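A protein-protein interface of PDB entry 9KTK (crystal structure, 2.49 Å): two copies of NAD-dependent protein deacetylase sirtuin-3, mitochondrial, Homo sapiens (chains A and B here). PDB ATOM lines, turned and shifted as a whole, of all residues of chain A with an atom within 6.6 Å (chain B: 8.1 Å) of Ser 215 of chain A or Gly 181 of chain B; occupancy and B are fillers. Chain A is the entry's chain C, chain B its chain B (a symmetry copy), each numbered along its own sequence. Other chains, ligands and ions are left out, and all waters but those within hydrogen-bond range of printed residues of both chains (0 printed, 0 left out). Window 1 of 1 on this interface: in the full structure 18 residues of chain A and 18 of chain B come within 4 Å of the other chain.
Leu 184 of chain B touches His 191 of chain A (CD1 to O, 3.8 Å). OE2 of Glu 67 of chain B touches CB of Glu 211 of chain A, 3.2 Å away. Glu 211 of chain A touches Pro 69 of chain B (CG to CG, 3.5 Å). Tyr 61 of chain B touches Pro 212 of chain A. Pro 212 of chain A touches Glu 67 of chain B. OG of Ser 215 of chain A touches CA of Gly 181 of chain B, at 3.5 Å. Leu 184 of chain B touches Ala 219 of chain A.
Of the 14 printed residues of chain B, 5 touch a printed residue of chain A. Hydrophobic or aromatic side chains of chain B that line the printed part of chain A: Tyr 61, Pro 69 and Leu 184. Of the 16 printed residues of chain A, 5 touch a printed residue of chain B. Hydrophobic or aromatic side chains of chain A within 4 Å of the printed part of chain B: Pro 212 and Ala 219. Among the printed residues, 7 pairs touch across the chains. Among the printed residues, no Asp or Glu carboxylate lies within 4 Å of a Lys or Arg side-chain nitrogen of the other chain.
Of chain A, only Ser 215 comes within 4 Å of Gly 181 of chain B. Of the printed residues of chain B, His 191 of chain A touches Leu 184. Of the printed residues of chain A, Pro 69 of chain B touches Glu 211. Of the printed residues of chain A, Glu 67 of chain B touches Glu 211 and Pro 212. Thr 217 of chain A touches none of the printed residues of chain B. Phe 66 of chain B touches none of the printed residues of chain A. The nearest residue of chain B that does not touch Ser 215 of chain A is Phe 180 of chain B (4.1 Å).
No position is printed for both chains. Of the 7 pairs that touch across the chains among the printed residues, none has its exchanged pair printed and touching as well.
The side-chain carboxylate of Glu 211 of chain A lies within hydrogen-bond range of the backbone NH of Ala 214 of chain A, 3.3 Å away. OE1 of Glu 211 of chain A is in hydrogen-bond range of N of Ser 215 of chain A (2.5 Å). The side-chain carboxylate (OE2) of Glu 67 of chain B lies close to the side-chain hydroxyl (OH) of Tyr 61 of chain B, at 3.3 Å.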
ATOM      1  N   MET A  29       7.593 -27.553  -3.011  1.00  0.00           N
ATOM      2  CA  MET A  29       7.934 -28.145  -1.714  1.00  0.00           C
ATOM      3  C   MET A  29       7.155 -29.441  -1.496  1.00  0.00           C
ATOM      4  O   MET A  29       5.919 -29.461  -1.621  1.00  0.00           O
ATOM      5  CB  MET A  29       7.678 -27.152  -0.557  1.00  0.00           C
ATOM      6  CG  MET A  29       7.971 -25.681  -0.892  1.00  0.00           C
ATOM      7  SD  MET A  29       7.539 -24.503   0.399  1.00  0.00           S
ATOM      8  CE  MET A  29       8.110 -25.416   1.853  1.00  0.00           C
ATOM      9  N   HIS A 191      17.127 -20.717  -1.997  1.00  0.00           N
ATOM     10  CA  HIS A 191      15.795 -20.148  -1.963  1.00  0.00           C
ATOM     11  C   HIS A 191      15.848 -18.643  -1.984  1.00  0.00           C
ATOM     12  O   HIS A 191      14.875 -18.016  -2.416  1.00  0.00           O
ATOM     13  CB  HIS A 191      15.003 -20.678  -0.750  1.00  0.00           C
ATOM     14  CG  HIS A 191      15.149 -19.870   0.508  1.00  0.00           C
ATOM     15  ND1 HIS A 191      15.978 -20.251   1.546  1.00  0.00           N
ATOM     16  CD2 HIS A 191      14.534 -18.732   0.919  1.00  0.00           C
ATOM     17  CE1 HIS A 191      15.889 -19.367   2.527  1.00  0.00           C
ATOM     18  NE2 HIS A 191      15.012 -18.440   2.174  1.00  0.00           N
ATOM     19  N   PHE A 195      12.759 -18.438  -4.834  1.00  0.00           N
ATOM     20  CA  PHE A 195      11.366 -18.115  -4.528  1.00  0.00           C
ATOM     21  C   PHE A 195      10.943 -16.731  -5.017  1.00  0.00           C
ATOM     22  O   PHE A 195       9.872 -16.627  -5.645  1.00  0.00           O
ATOM     23  CB  PHE A 195      11.129 -18.261  -3.027  1.00  0.00           C
ATOM     24  CG  PHE A 195      10.931 -19.671  -2.578  1.00  0.00           C
ATOM     25  CD1 PHE A 195      11.959 -20.606  -2.686  1.00  0.00           C
ATOM     26  CD2 PHE A 195       9.717 -20.061  -2.007  1.00  0.00           C
ATOM     27  CE1 PHE A 195      11.786 -21.905  -2.238  1.00  0.00           C
ATOM     28  CE2 PHE A 195       9.531 -21.367  -1.566  1.00  0.00           C
ATOM     29  CZ  PHE A 195      10.572 -22.295  -1.681  1.00  0.00           C
ATOM     30  N   LEU A 208       4.291 -29.184   7.105  1.00  0.00           N
ATOM     31  CA  LEU A 208       4.793 -27.817   7.283  1.00  0.00           C
ATOM     32  C   LEU A 208       5.050 -27.528   8.762  1.00  0.00           C
ATOM     33  O   LEU A 208       4.793 -26.429   9.258  1.00  0.00           O
ATOM     34  CB  LEU A 208       3.838 -26.785   6.673  1.00  0.00           C
ATOM     35  CG  LEU A 208       3.677 -26.725   5.153  1.00  0.00           C
ATOM     36  CD1 LEU A 208       2.973 -25.438   4.734  1.00  0.00           C
ATOM     37  CD2 LEU A 208       5.027 -26.843   4.456  1.00  0.00           C
ATOM     38  N   VAL A 210       8.167 -28.631  10.628  1.00  0.00           N
ATOM     39  CA  VAL A 210       9.574 -28.376  10.948  1.00  0.00           C
ATOM     40  C   VAL A 210      10.075 -27.170  10.154  1.00  0.00           C
ATOM     41  O   VAL A 210       9.959 -27.096   8.921  1.00  0.00           O
ATOM     42  CB  VAL A 210      10.467 -29.619  10.733  1.00  0.00           C
ATOM     43  CG1 VAL A 210      10.605 -29.970   9.299  1.00  0.00           C
ATOM     44  CG2 VAL A 210      11.874 -29.374  11.284  1.00  0.00           C
ATOM     45  N   GLU A 211      10.582 -26.204  10.887  1.00  0.00           N
ATOM     46  CA  GLU A 211      11.312 -25.089  10.336  1.00  0.00           C
ATOM     47  C   GLU A 211      12.773 -25.519  10.190  1.00  0.00           C
ATOM     48  O   GLU A 211      13.207 -26.488  10.816  1.00  0.00           O
ATOM     49  CB  GLU A 211      11.130 -23.876  11.247  1.00  0.00           C
ATOM     50  CG  GLU A 211       9.695 -23.285  11.229  1.00  0.00           C
ATOM     51  CD  GLU A 211       9.346 -22.519   9.958  1.00  0.00           C
ATOM     52  OE1 GLU A 211      10.146 -22.552   8.999  1.00  0.00           O
ATOM     53  OE2 GLU A 211       8.263 -21.886   9.902  1.00  0.00           O
ATOM     54  N   PRO A 212      13.546 -24.867   9.314  1.00  0.00           N
ATOM     55  CA  PRO A 212      13.238 -23.689   8.498  1.00  0.00           C
ATOM     56  C   PRO A 212      12.511 -24.050   7.225  1.00  0.00           C
ATOM     57  O   PRO A 212      12.165 -23.152   6.459  1.00  0.00           O
ATOM     58  CB  PRO A 212      14.627 -23.082   8.253  1.00  0.00           C
ATOM     59  CG  PRO A 212      15.511 -24.287   8.160  1.00  0.00           C
ATOM     60  CD  PRO A 212      14.921 -25.337   9.083  1.00  0.00           C
ATOM     61  N   PHE A 213      12.234 -25.338   7.001  1.00  0.00           N
ATOM     62  CA  PHE A 213      11.448 -25.745   5.837  1.00  0.00           C
ATOM     63  C   PHE A 213      10.094 -25.046   5.765  1.00  0.00           C
ATOM     64  O   PHE A 213       9.687 -24.568   4.703  1.00  0.00           O
ATOM     65  CB  PHE A 213      11.261 -27.260   5.823  1.00  0.00           C
ATOM     66  CG  PHE A 213      10.796 -27.791   4.488  1.00  0.00           C
ATOM     67  CD1 PHE A 213       9.442 -27.887   4.185  1.00  0.00           C
ATOM     68  CD2 PHE A 213      11.709 -28.121   3.511  1.00  0.00           C
ATOM     69  CE1 PHE A 213       9.008 -28.361   2.952  1.00  0.00           C
ATOM     70  CE2 PHE A 213      11.285 -28.593   2.267  1.00  0.00           C
ATOM     71  CZ  PHE A 213       9.927 -28.707   1.989  1.00  0.00           C
ATOM     72  N   ALA A 214       9.368 -25.000   6.874  1.00  0.00           N
ATOM     73  CA  ALA A 214       7.999 -24.502   6.828  1.00  0.00           C
ATOM     74  C   ALA A 214       7.936 -23.033   6.405  1.00  0.00           C
ATOM     75  O   ALA A 214       6.974 -22.614   5.738  1.00  0.00           O
ATOM     76  CB  ALA A 214       7.329 -24.709   8.189  1.00  0.00           C
ATOM     77  N   SER A 215       8.946 -22.240   6.792  1.00  0.00           N
ATOM     78  CA  SER A 215       8.972 -20.812   6.470  1.00  0.00           C
ATOM     79  C   SER A 215       9.061 -20.517   4.977  1.00  0.00           C
ATOM     80  O   SER A 215       8.690 -19.407   4.561  1.00  0.00           O
ATOM     81  CB  SER A 215      10.135 -20.102   7.184  1.00  0.00           C
ATOM     82  OG  SER A 215       9.917 -20.016   8.588  1.00  0.00           O
ATOM     83  N   LEU A 216       9.532 -21.461   4.158  1.00  0.00           N
ATOM     84  CA  LEU A 216       9.708 -21.122   2.755  1.00  0.00           C
ATOM     85  C   LEU A 216       8.406 -20.696   2.104  1.00  0.00           C
ATOM     86  O   LEU A 216       8.441 -19.949   1.119  1.00  0.00           O
ATOM     87  CB  LEU A 216      10.332 -22.277   1.988  1.00  0.00           C
ATOM     88  CG  LEU A 216      11.784 -22.415   2.450  1.00  0.00           C
ATOM     89  CD1 LEU A 216      11.977 -23.738   3.087  1.00  0.00           C
ATOM     90  CD2 LEU A 216      12.783 -22.199   1.362  1.00  0.00           C
ATOM     91  N   THR A 217       7.269 -21.115   2.674  1.00  0.00           N
ATOM     92  CA  THR A 217       5.947 -20.807   2.137  1.00  0.00           C
ATOM     93  C   THR A 217       5.694 -19.309   1.983  1.00  0.00           C
ATOM     94  O   THR A 217       4.861 -18.898   1.164  1.00  0.00           O
ATOM     95  CB  THR A 217       4.886 -21.403   3.052  1.00  0.00           C
ATOM     96  OG1 THR A 217       5.070 -20.875   4.379  1.00  0.00           O
ATOM     97  CG2 THR A 217       4.989 -22.918   3.057  1.00  0.00           C
ATOM     98  N   GLU A 218       6.364 -18.477   2.762  1.00  0.00           N
ATOM     99  CA  GLU A 218       6.096 -17.056   2.685  1.00  0.00           C
ATOM    100  C   GLU A 218       7.151 -16.316   1.878  1.00  0.00           C
ATOM    101  O   GLU A 218       6.988 -15.117   1.602  1.00  0.00           O
ATOM    102  CB  GLU A 218       5.972 -16.481   4.092  1.00  0.00           C
ATOM    103  CG  GLU A 218       4.709 -16.949   4.794  1.00  0.00           C
ATOM    104  CD  GLU A 218       4.952 -17.208   6.255  1.00  0.00           C
ATOM    105  OE1 GLU A 218       5.928 -17.938   6.552  1.00  0.00           O
ATOM    106  OE2 GLU A 218       4.186 -16.664   7.100  1.00  0.00           O
ATOM    107  N   ALA A 219       8.192 -17.028   1.444  1.00  0.00           N
ATOM    108  CA  ALA A 219       9.277 -16.478   0.649  1.00  0.00           C
ATOM    109  C   ALA A 219       8.869 -16.115  -0.772  1.00  0.00           C
ATOM    110  O   ALA A 219       9.682 -15.516  -1.493  1.00  0.00           O
ATOM    111  CB  ALA A 219      10.435 -17.481   0.597  1.00  0.00           C
ATOM    112  N   VAL A 220       7.669 -16.472  -1.213  1.00  0.00           N
ATOM    113  CA  VAL A 220       7.262 -16.069  -2.549  1.00  0.00           C
ATOM    114  C   VAL A 220       6.671 -14.674  -2.460  1.00  0.00           C
ATOM    115  O   VAL A 220       6.164 -14.263  -1.410  1.00  0.00           O
ATOM    116  CB  VAL A 220       6.279 -17.075  -3.178  1.00  0.00           C
ATOM    117  CG1 VAL A 220       6.900 -18.433  -3.251  1.00  0.00           C
ATOM    118  CG2 VAL A 220       4.992 -17.141  -2.371  1.00  0.00           C
ATOM    119  N   PRO A 236       1.733 -22.306   7.429  1.00  0.00           N
ATOM    120  CA  PRO A 236       1.428 -20.887   7.196  1.00  0.00           C
ATOM    121  C   PRO A 236       0.306 -20.645   6.200  1.00  0.00           C
ATOM    122  O   PRO A 236      -0.046 -19.483   5.957  1.00  0.00           O
ATOM    123  CB  PRO A 236       2.767 -20.326   6.688  1.00  0.00           C
ATOM    124  CG  PRO A 236       3.804 -21.300   7.226  1.00  0.00           C
ATOM    125  CD  PRO A 236       3.124 -22.631   7.071  1.00  0.00           C
ATOM    126  N   TYR B  61      20.603 -26.675  14.837  1.00  0.00           N
ATOM    127  CA  TYR B  61      21.612 -26.490  13.796  1.00  0.00           C
ATOM    128  C   TYR B  61      22.236 -25.115  14.005  1.00  0.00           C
ATOM    129  O   TYR B  61      21.554 -24.205  14.493  1.00  0.00           O
ATOM    130  CB  TYR B  61      21.020 -26.639  12.370  1.00  0.00           C
ATOM    131  CG  TYR B  61      19.883 -25.686  12.069  1.00  0.00           C
ATOM    132  CD1 TYR B  61      18.599 -25.981  12.475  1.00  0.00           C
ATOM    133  CD2 TYR B  61      20.107 -24.466  11.439  1.00  0.00           C
ATOM    134  CE1 TYR B  61      17.560 -25.135  12.245  1.00  0.00           C
ATOM    135  CE2 TYR B  61      19.049 -23.578  11.212  1.00  0.00           C
ATOM    136  CZ  TYR B  61      17.764 -23.935  11.628  1.00  0.00           C
ATOM    137  OH  TYR B  61      16.658 -23.122  11.445  1.00  0.00           O
ATOM    138  N   PHE B  66      19.565 -17.449  13.309  1.00  0.00           N
ATOM    139  CA  PHE B  66      18.841 -16.602  12.360  1.00  0.00           C
ATOM    140  C   PHE B  66      17.518 -17.234  11.925  1.00  0.00           C
ATOM    141  O   PHE B  66      16.942 -16.850  10.904  1.00  0.00           O
ATOM    142  CB  PHE B  66      19.693 -16.277  11.125  1.00  0.00           C
ATOM    143  CG  PHE B  66      21.146 -16.128  11.402  1.00  0.00           C
ATOM    144  CD1 PHE B  66      21.645 -14.951  11.975  1.00  0.00           C
ATOM    145  CD2 PHE B  66      22.031 -17.141  11.074  1.00  0.00           C
ATOM    146  CE1 PHE B  66      23.014 -14.797  12.213  1.00  0.00           C
ATOM    147  CE2 PHE B  66      23.422 -16.994  11.302  1.00  0.00           C
ATOM    148  CZ  PHE B  66      23.911 -15.814  11.872  1.00  0.00           C
ATOM    149  N   GLU B  67      17.021 -18.189  12.681  1.00  0.00           N
ATOM    150  CA  GLU B  67      15.733 -18.810  12.402  1.00  0.00           C
ATOM    151  C   GLU B  67      14.613 -18.106  13.193  1.00  0.00           C
ATOM    152  O   GLU B  67      14.700 -17.950  14.413  1.00  0.00           O
ATOM    153  CB  GLU B  67      15.904 -20.283  12.740  1.00  0.00           C
ATOM    154  CG  GLU B  67      14.794 -21.021  13.361  1.00  0.00           C
ATOM    155  CD  GLU B  67      14.016 -21.808  12.438  1.00  0.00           C
ATOM    156  OE1 GLU B  67      13.802 -21.354  11.294  1.00  0.00           O
ATOM    157  OE2 GLU B  67      13.729 -22.935  12.862  1.00  0.00           O
ATOM    158  N   LEU B  68      13.590 -17.617  12.494  1.00  0.00           N
ATOM    159  CA  LEU B  68      12.606 -16.758  13.162  1.00  0.00           C
ATOM    160  C   LEU B  68      11.741 -17.460  14.223  1.00  0.00           C
ATOM    161  O   LEU B  68      11.439 -16.835  15.252  1.00  0.00           O
ATOM    162  CB  LEU B  68      11.699 -16.065  12.134  1.00  0.00           C
ATOM    163  CG  LEU B  68      10.792 -14.988  12.776  1.00  0.00           C
ATOM    164  CD1 LEU B  68      11.589 -13.910  13.449  1.00  0.00           C
ATOM    165  CD2 LEU B  68       9.809 -14.344  11.835  1.00  0.00           C
ATOM    166  N   PRO B  69      11.302 -18.733  14.047  1.00  0.00           N
ATOM    167  CA  PRO B  69      10.499 -19.345  15.117  1.00  0.00           C
ATOM    168  C   PRO B  69      11.351 -19.854  16.264  1.00  0.00           C
ATOM    169  O   PRO B  69      10.869 -19.896  17.404  1.00  0.00           O
ATOM    170  CB  PRO B  69       9.738 -20.484  14.416  1.00  0.00           C
ATOM    171  CG  PRO B  69       9.884 -20.228  12.961  1.00  0.00           C
ATOM    172  CD  PRO B  69      11.198 -19.506  12.795  1.00  0.00           C
ATOM    173  N   PHE B  70      12.603 -20.240  15.995  1.00  0.00           N
ATOM    174  CA  PHE B  70      13.538 -20.442  17.102  1.00  0.00           C
ATOM    175  C   PHE B  70      13.643 -19.179  17.951  1.00  0.00           C
ATOM    176  O   PHE B  70      13.578 -19.242  19.181  1.00  0.00           O
ATOM    177  CB  PHE B  70      14.926 -20.859  16.585  1.00  0.00           C
ATOM    178  CG  PHE B  70      15.788 -21.516  17.627  1.00  0.00           C
ATOM    179  CD1 PHE B  70      15.639 -22.864  17.930  1.00  0.00           C
ATOM    180  CD2 PHE B  70      16.719 -20.772  18.341  1.00  0.00           C
ATOM    181  CE1 PHE B  70      16.420 -23.467  18.911  1.00  0.00           C
ATOM    182  CE2 PHE B  70      17.496 -21.366  19.334  1.00  0.00           C
ATOM    183  CZ  PHE B  70      17.355 -22.715  19.606  1.00  0.00           C
ATOM    184  N   PHE B  72      11.529 -16.919  18.751  1.00  0.00           N
ATOM    185  CA  PHE B  72      10.458 -16.822  19.768  1.00  0.00           C
ATOM    186  C   PHE B  72      10.492 -18.020  20.731  1.00  0.00           C
ATOM    187  O   PHE B  72       9.563 -18.822  20.801  1.00  0.00           O
ATOM    188  CB  PHE B  72       9.077 -16.779  19.132  1.00  0.00           C
ATOM    189  CG  PHE B  72       8.937 -15.921  17.939  1.00  0.00           C
ATOM    190  CD1 PHE B  72       9.604 -14.731  17.808  1.00  0.00           C
ATOM    191  CD2 PHE B  72       8.062 -16.314  16.932  1.00  0.00           C
ATOM    192  CE1 PHE B  72       9.411 -13.941  16.674  1.00  0.00           C
ATOM    193  CE2 PHE B  72       7.863 -15.541  15.800  1.00  0.00           C
ATOM    194  CZ  PHE B  72       8.539 -14.353  15.667  1.00  0.00           C
ATOM    195  N   VAL B 178      18.220 -10.463   8.430  1.00  0.00           N
ATOM    196  CA  VAL B 178      17.267 -11.291   7.705  1.00  0.00           C
ATOM    197  C   VAL B 178      17.273 -12.700   8.279  1.00  0.00           C
ATOM    198  O   VAL B 178      18.315 -13.368   8.327  1.00  0.00           O
ATOM    199  CB  VAL B 178      17.580 -11.300   6.209  1.00  0.00           C
ATOM    200  CG1 VAL B 178      16.638 -12.238   5.513  1.00  0.00           C
ATOM    201  CG2 VAL B 178      17.438  -9.907   5.668  1.00  0.00           C
ATOM    202  N   PHE B 179      16.099 -13.155   8.712  1.00  0.00           N
ATOM    203  CA  PHE B 179      15.928 -14.460   9.327  1.00  0.00           C
ATOM    204  C   PHE B 179      15.179 -15.362   8.356  1.00  0.00           C
ATOM    205  O   PHE B 179      14.315 -14.883   7.603  1.00  0.00           O
ATOM    206  CB  PHE B 179      15.123 -14.344  10.629  1.00  0.00           C
ATOM    207  CG  PHE B 179      15.946 -14.064  11.835  1.00  0.00           C
ATOM    208  CD1 PHE B 179      17.204 -13.444  11.715  1.00  0.00           C
ATOM    209  CD2 PHE B 179      15.479 -14.396  13.088  1.00  0.00           C
ATOM    210  CE1 PHE B 179      17.984 -13.169  12.857  1.00  0.00           C
ATOM    211  CE2 PHE B 179      16.243 -14.135  14.226  1.00  0.00           C
ATOM    212  CZ  PHE B 179      17.489 -13.518  14.115  1.00  0.00           C
ATOM    213  N   PHE B 180      15.489 -16.660   8.368  1.00  0.00           N
ATOM    214  CA  PHE B 180      14.514 -17.575   7.777  1.00  0.00           C
ATOM    215  C   PHE B 180      13.164 -17.396   8.482  1.00  0.00           C
ATOM    216  O   PHE B 180      13.044 -17.618   9.692  1.00  0.00           O
ATOM    217  CB  PHE B 180      14.918 -19.051   7.852  1.00  0.00           C
ATOM    218  CG  PHE B 180      16.372 -19.315   7.822  1.00  0.00           C
ATOM    219  CD1 PHE B 180      17.078 -19.298   6.617  1.00  0.00           C
ATOM    220  CD2 PHE B 180      17.031 -19.724   8.981  1.00  0.00           C
ATOM    221  CE1 PHE B 180      18.446 -19.595   6.603  1.00  0.00           C
ATOM    222  CE2 PHE B 180      18.398 -20.049   8.967  1.00  0.00           C
ATOM    223  CZ  PHE B 180      19.098 -19.980   7.778  1.00  0.00           C
ATOM    224  N   GLY B 181      12.136 -17.000   7.738  1.00  0.00           N
ATOM    225  CA  GLY B 181      10.863 -16.651   8.331  1.00  0.00           C
ATOM    226  C   GLY B 181      10.480 -15.222   8.008  1.00  0.00           C
ATOM    227  O   GLY B 181       9.321 -14.925   7.708  1.00  0.00           O
ATOM    228  N   GLU B 182      11.450 -14.326   8.071  1.00  0.00           N
ATOM    229  CA  GLU B 182      11.235 -12.982   7.569  1.00  0.00           C
ATOM    230  C   GLU B 182      11.284 -12.986   6.043  1.00  0.00           C
ATOM    231  O   GLU B 182      12.155 -13.646   5.459  1.00  0.00           O
ATOM    232  CB  GLU B 182      12.311 -12.054   8.097  1.00  0.00           C
ATOM    233  CG  GLU B 182      12.367 -11.983   9.586  1.00  0.00           C
ATOM    234  CD  GLU B 182      12.969 -10.696  10.070  1.00  0.00           C
ATOM    235  OE1 GLU B 182      13.675 -10.017   9.283  1.00  0.00           O
ATOM    236  OE2 GLU B 182      12.745 -10.363  11.248  1.00  0.00           O
ATOM    237  N   PRO B 183      10.394 -12.236   5.383  1.00  0.00           N
ATOM    238  CA  PRO B 183      10.443 -12.130   3.911  1.00  0.00           C
ATOM    239  C   PRO B 183      11.734 -11.466   3.440  1.00  0.00           C
ATOM    240  O   PRO B 183      12.136 -10.437   3.974  1.00  0.00           O
ATOM    241  CB  PRO B 183       9.216 -11.267   3.580  1.00  0.00           C
ATOM    242  CG  PRO B 183       9.021 -10.374   4.837  1.00  0.00           C
ATOM    243  CD  PRO B 183       9.444 -11.278   5.997  1.00  0.00           C
ATOM    244  N   LEU B 184      12.354 -12.043   2.408  1.00  0.00           N
ATOM    245  CA  LEU B 184      13.757 -11.824   2.036  1.00  0.00           C
ATOM    246  C   LEU B 184      13.950 -10.474   1.309  1.00  0.00           C
ATOM    247  O   LEU B 184      12.974  -9.891   0.821  1.00  0.00           O
ATOM    248  CB  LEU B 184      14.240 -13.052   1.238  1.00  0.00           C
ATOM    249  CG  LEU B 184      13.468 -13.709   0.070  1.00  0.00           C
ATOM    250  CD1 LEU B 184      14.300 -14.802  -0.544  1.00  0.00           C
ATOM    251  CD2 LEU B 184      12.121 -14.321   0.433  1.00  0.00           C
